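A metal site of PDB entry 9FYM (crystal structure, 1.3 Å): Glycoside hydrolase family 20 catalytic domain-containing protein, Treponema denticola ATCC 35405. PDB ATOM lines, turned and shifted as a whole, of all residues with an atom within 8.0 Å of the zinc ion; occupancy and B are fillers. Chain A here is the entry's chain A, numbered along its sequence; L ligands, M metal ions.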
ATOM      1  N   ASN A  93       3.810  -6.810 -22.556  1.00  0.00           N
ATOM      2  CA  ASN A  93       4.039  -7.016 -21.129  1.00  0.00           C
ATOM      3  C   ASN A  93       5.448  -6.584 -20.766  1.00  0.00           C
ATOM      4  O   ASN A  93       6.424  -7.195 -21.202  1.00  0.00           O
ATOM      5  CB  ASN A  93       3.775  -8.437 -20.643  1.00  0.00           C
ATOM      6  CG  ASN A  93       3.537  -8.475 -19.133  1.00  0.00           C
ATOM      7  OD1 ASN A  93       4.118  -7.661 -18.398  1.00  0.00           O
ATOM      8  ND2 ASN A  93       2.698  -9.410 -18.678  1.00  0.00           N
ATOM      9  N   GLY A  96       6.134  -9.060 -16.732  1.00  0.00           N
ATOM     10  CA  GLY A  96       5.717 -10.435 -16.573  1.00  0.00           C
ATOM     11  C   GLY A  96       5.578 -11.125 -17.920  1.00  0.00           C
ATOM     12  O   GLY A  96       5.909 -10.594 -18.978  1.00  0.00           O
ATOM     13  N   HIS A  97       5.120 -12.375 -17.858  1.00  0.00           N
ATOM     14  CA  HIS A  97       4.900 -13.224 -19.036  1.00  0.00           C
ATOM     15  C   HIS A  97       6.061 -13.134 -20.035  1.00  0.00           C
ATOM     16  O   HIS A  97       5.904 -12.774 -21.199  1.00  0.00           O
ATOM     17  CB  HIS A  97       3.573 -12.882 -19.692  1.00  0.00           C
ATOM     18  CG  HIS A  97       3.089 -13.915 -20.662  1.00  0.00           C
ATOM     19  ND1 HIS A  97       2.785 -15.210 -20.273  1.00  0.00           N
ATOM     20  CD2 HIS A  97       2.886 -13.853 -22.001  1.00  0.00           C
ATOM     21  CE1 HIS A  97       2.408 -15.898 -21.342  1.00  0.00           C
ATOM     22  NE2 HIS A  97       2.467 -15.095 -22.401  1.00  0.00           N
ATOM     23  N   GLN A  98       7.217 -13.509 -19.565  1.00  0.00           N
ATOM     24  CA  GLN A  98       8.444 -13.468 -20.391  1.00  0.00           C
ATOM     25  C   GLN A  98       8.786 -14.824 -20.990  1.00  0.00           C
ATOM     26  O   GLN A  98       9.826 -14.984 -21.643  1.00  0.00           O
ATOM     27  CB  GLN A  98       9.617 -12.905 -19.618  1.00  0.00           C
ATOM     28  CG  GLN A  98       9.332 -11.491 -19.099  1.00  0.00           C
ATOM     29  CD  GLN A  98       9.286 -10.448 -20.200  1.00  0.00           C
ATOM     30  OE1 GLN A  98      10.140 -10.438 -21.060  1.00  0.00           O
ATOM     31  NE2 GLN A  98       8.244  -9.617 -20.177  1.00  0.00           N
ATOM     32  N   SER A  99       7.916 -15.795 -20.752  1.00  0.00           N
ATOM     33  CA  SER A  99       8.023 -17.151 -21.254  1.00  0.00           C
ATOM     34  C   SER A  99       6.650 -17.792 -21.257  1.00  0.00           C
ATOM     35  O   SER A  99       5.674 -17.246 -20.726  1.00  0.00           O
ATOM     36  CB  SER A  99       8.995 -17.912 -20.345  1.00  0.00           C
ATOM     37  OG  SER A  99       8.365 -18.187 -19.093  1.00  0.00           O
ATOM     38  N   TRP A 100       6.544 -18.930 -21.941  1.00  0.00           N
ATOM     39  CA  TRP A 100       5.312 -19.723 -21.921  1.00  0.00           C
ATOM     40  C   TRP A 100       5.725 -21.186 -22.073  1.00  0.00           C
ATOM     41  O   TRP A 100       6.469 -21.525 -22.982  1.00  0.00           O
ATOM     42  CB  TRP A 100       4.407 -19.284 -23.061  1.00  0.00           C
ATOM     43  CG  TRP A 100       3.203 -20.107 -23.242  1.00  0.00           C
ATOM     44  CD1 TRP A 100       1.984 -19.929 -22.641  1.00  0.00           C
ATOM     45  CD2 TRP A 100       3.044 -21.164 -24.172  1.00  0.00           C
ATOM     46  NE1 TRP A 100       1.098 -20.862 -23.106  1.00  0.00           N
ATOM     47  CE2 TRP A 100       1.719 -21.635 -24.050  1.00  0.00           C
ATOM     48  CE3 TRP A 100       3.898 -21.785 -25.088  1.00  0.00           C
ATOM     49  CZ2 TRP A 100       1.240 -22.669 -24.813  1.00  0.00           C
ATOM     50  CZ3 TRP A 100       3.421 -22.835 -25.832  1.00  0.00           C
ATOM     51  CH2 TRP A 100       2.103 -23.273 -25.687  1.00  0.00           C
ATOM     52  N   GLU A 101       5.250 -22.044 -21.166  1.00  0.00           N
ATOM     53  CA  GLU A 101       5.670 -23.454 -21.166  1.00  0.00           C
ATOM     54  C   GLU A 101       7.208 -23.465 -21.185  1.00  0.00           C
ATOM     55  O   GLU A 101       7.843 -22.741 -20.405  1.00  0.00           O
ATOM     56  CB  GLU A 101       4.980 -24.168 -22.317  1.00  0.00           C
ATOM     57  CG  GLU A 101       3.459 -24.226 -22.198  1.00  0.00           C
ATOM     58  CD  GLU A 101       3.009 -25.204 -21.125  1.00  0.00           C
ATOM     59  OE1 GLU A 101       3.772 -26.163 -20.835  1.00  0.00           O
ATOM     60  OE2 GLU A 101       1.909 -25.001 -20.575  1.00  0.00           O
ATOM     61  N   PHE A 105      10.808 -16.137 -24.179  1.00  0.00           N
ATOM     62  CA  PHE A 105      10.543 -15.168 -25.228  1.00  0.00           C
ATOM     63  C   PHE A 105      11.787 -14.356 -25.563  1.00  0.00           C
ATOM     64  O   PHE A 105      12.852 -14.471 -24.938  1.00  0.00           O
ATOM     65  CB  PHE A 105       9.341 -14.276 -24.889  1.00  0.00           C
ATOM     66  CG  PHE A 105       8.021 -15.021 -24.723  1.00  0.00           C
ATOM     67  CD1 PHE A 105       7.734 -16.196 -25.402  1.00  0.00           C
ATOM     68  CD2 PHE A 105       7.065 -14.508 -23.887  1.00  0.00           C
ATOM     69  CE1 PHE A 105       6.503 -16.814 -25.285  1.00  0.00           C
ATOM     70  CE2 PHE A 105       5.842 -15.130 -23.742  1.00  0.00           C
ATOM     71  CZ  PHE A 105       5.566 -16.291 -24.443  1.00  0.00           C
ATOM     72  N   ILE A 127       7.308 -22.956 -12.417  1.00  0.00           N
ATOM     73  CA  ILE A 127       6.833 -21.582 -12.448  1.00  0.00           C
ATOM     74  C   ILE A 127       5.843 -21.443 -13.595  1.00  0.00           C
ATOM     75  O   ILE A 127       5.881 -22.217 -14.563  1.00  0.00           O
ATOM     76  CB  ILE A 127       7.990 -20.558 -12.582  1.00  0.00           C
ATOM     77  CG1 ILE A 127       8.796 -20.827 -13.876  1.00  0.00           C
ATOM     78  CG2 ILE A 127       8.871 -20.582 -11.357  1.00  0.00           C
ATOM     79  CD1 ILE A 127       9.751 -19.682 -14.209  1.00  0.00           C
ATOM     80  N   TYR A 128       4.912 -20.493 -13.472  1.00  0.00           N
ATOM     81  CA  TYR A 128       4.013 -20.218 -14.573  1.00  0.00           C
ATOM     82  C   TYR A 128       4.776 -19.602 -15.743  1.00  0.00           C
ATOM     83  O   TYR A 128       4.706 -20.076 -16.879  1.00  0.00           O
ATOM     84  CB  TYR A 128       2.892 -19.282 -14.104  1.00  0.00           C
ATOM     85  CG  TYR A 128       1.875 -19.956 -13.196  1.00  0.00           C
ATOM     86  CD1 TYR A 128       0.887 -20.786 -13.722  1.00  0.00           C
ATOM     87  CD2 TYR A 128       1.929 -19.794 -11.815  1.00  0.00           C
ATOM     88  CE1 TYR A 128      -0.043 -21.411 -12.884  1.00  0.00           C
ATOM     89  CE2 TYR A 128       1.021 -20.417 -10.983  1.00  0.00           C
ATOM     90  CZ  TYR A 128       0.041 -21.227 -11.520  1.00  0.00           C
ATOM     91  OH  TYR A 128      -0.875 -21.854 -10.686  1.00  0.00           O
ATOM     92  N   CYS A 129       5.581 -18.579 -15.452  1.00  0.00           N
ATOM     93  CA  CYS A 129       6.360 -17.889 -16.479  1.00  0.00           C
ATOM     94  C   CYS A 129       7.354 -16.969 -15.805  1.00  0.00           C
ATOM     95  O   CYS A 129       7.245 -16.652 -14.619  1.00  0.00           O
ATOM     96  CB  CYS A 129       5.444 -17.150 -17.480  1.00  0.00           C
ATOM     97  SG  CYS A 129       4.435 -15.863 -16.690  1.00  0.00           S
ATOM     98  N   ARG A 130       8.362 -16.557 -16.580  1.00  0.00           N
ATOM     99  CA  ARG A 130       9.466 -15.762 -16.070  1.00  0.00           C
ATOM    100  C   ARG A 130       9.112 -14.282 -16.057  1.00  0.00           C
ATOM    101  O   ARG A 130       8.165 -13.848 -16.746  1.00  0.00           O
ATOM    102  CB  ARG A 130      10.718 -15.921 -16.940  1.00  0.00           C
ATOM    103  CG  ARG A 130      11.163 -17.383 -17.112  1.00  0.00           C
ATOM    104  CD  ARG A 130      12.529 -17.496 -17.799  1.00  0.00           C
ATOM    105  NE  ARG A 130      13.602 -17.535 -16.819  1.00  0.00           N
ATOM    106  CZ  ARG A 130      13.941 -18.609 -16.110  1.00  0.00           C
ATOM    107  NH1 ARG A 130      13.367 -19.790 -16.299  1.00  0.00           N
ATOM    108  NH2 ARG A 130      14.869 -18.493 -15.172  1.00  0.00           N
ATOM    109  N   ASP A 164       0.531  -8.007 -15.750  1.00  0.00           N
ATOM    110  CA  ASP A 164       0.053  -9.240 -15.114  1.00  0.00           C
ATOM    111  C   ASP A 164       1.145 -10.288 -15.234  1.00  0.00           C
ATOM    112  O   ASP A 164       2.208 -10.055 -15.829  1.00  0.00           O
ATOM    113  CB  ASP A 164      -1.240  -9.725 -15.748  1.00  0.00           C
ATOM    114  CG  ASP A 164      -1.104 -10.079 -17.230  1.00  0.00           C
ATOM    115  OD1 ASP A 164      -0.214  -9.572 -17.916  1.00  0.00           O
ATOM    116  OD2 ASP A 164      -1.982 -10.835 -17.747  1.00  0.00           O
ATOM    117  N   GLU A 165       0.883 -11.472 -14.695  1.00  0.00           N
ATOM    118  CA  GLU A 165       1.808 -12.593 -14.861  1.00  0.00           C
ATOM    119  C   GLU A 165       3.204 -12.232 -14.368  1.00  0.00           C
ATOM    120  O   GLU A 165       4.190 -12.676 -14.941  1.00  0.00           O
ATOM    121  CB  GLU A 165       1.878 -13.057 -16.309  1.00  0.00           C
ATOM    122  CG  GLU A 165       0.602 -13.431 -17.037  1.00  0.00           C
ATOM    123  CD  GLU A 165       0.115 -14.758 -16.579  1.00  0.00           C
ATOM    124  OE1 GLU A 165       0.725 -15.759 -17.038  1.00  0.00           O
ATOM    125  OE2 GLU A 165      -0.867 -14.819 -15.805  1.00  0.00           O
ATOM    126  N   VAL A 166       3.272 -11.471 -13.275  1.00  0.00           N
ATOM    127  CA  VAL A 166       4.532 -11.178 -12.586  1.00  0.00           C
ATOM    128  C   VAL A 166       4.532 -12.074 -11.347  1.00  0.00           C
ATOM    129  O   VAL A 166       3.890 -11.752 -10.343  1.00  0.00           O
ATOM    130  CB  VAL A 166       4.673  -9.705 -12.222  1.00  0.00           C
ATOM    131  CG1 VAL A 166       5.980  -9.512 -11.434  1.00  0.00           C
ATOM    132  CG2 VAL A 166       4.674  -8.837 -13.486  1.00  0.00           C
ATOM    133  N   PHE A 167       5.217 -13.207 -11.425  1.00  0.00           N
ATOM    134  CA  PHE A 167       5.241 -14.180 -10.319  1.00  0.00           C
ATOM    135  C   PHE A 167       6.571 -14.227  -9.602  1.00  0.00           C
ATOM    136  O   PHE A 167       6.693 -14.933  -8.592  1.00  0.00           O
ATOM    137  CB  PHE A 167       4.889 -15.557 -10.893  1.00  0.00           C
ATOM    138  CG  PHE A 167       3.528 -15.618 -11.511  1.00  0.00           C
ATOM    139  CD1 PHE A 167       2.383 -15.515 -10.721  1.00  0.00           C
ATOM    140  CD2 PHE A 167       3.378 -15.787 -12.855  1.00  0.00           C
ATOM    141  CE1 PHE A 167       1.118 -15.596 -11.285  1.00  0.00           C
ATOM    142  CE2 PHE A 167       2.118 -15.862 -13.431  1.00  0.00           C
ATOM    143  CZ  PHE A 167       0.992 -15.755 -12.656  1.00  0.00           C
HETATM  144  N1  LIG L   1       1.689 -20.340 -19.122  1.00  0.00           N
HETATM  145  C1  LIG L   1       2.397 -19.186 -19.016  1.00  0.00           C
HETATM  146  N2  LIG L   1       1.958 -18.488 -17.945  1.00  0.00           N
HETATM  147  C2  LIG L   1       0.962 -19.218 -17.365  1.00  0.00           C
HETATM  148  C3  LIG L   1       0.801 -20.382 -18.110  1.00  0.00           C
HETATM  149 ZN    ZN M   1       2.534 -16.026 -18.134  1.00  0.00          ZN
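Three residues have an atom within 4 Å of the zinc ion: His 97, Cys 129 and Glu 165. Along chain A the residues within 4 Å of the zinc ion span positions 97 to 165.
OE1 of Glu 165 binds the zinc ion (2.1 Å). ND1 of His 97 is bound to the zinc ion. The zinc ion is bound by SG of Cys 129. N2 of the ligand is bound to the zinc ion, at 2.5 Å.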
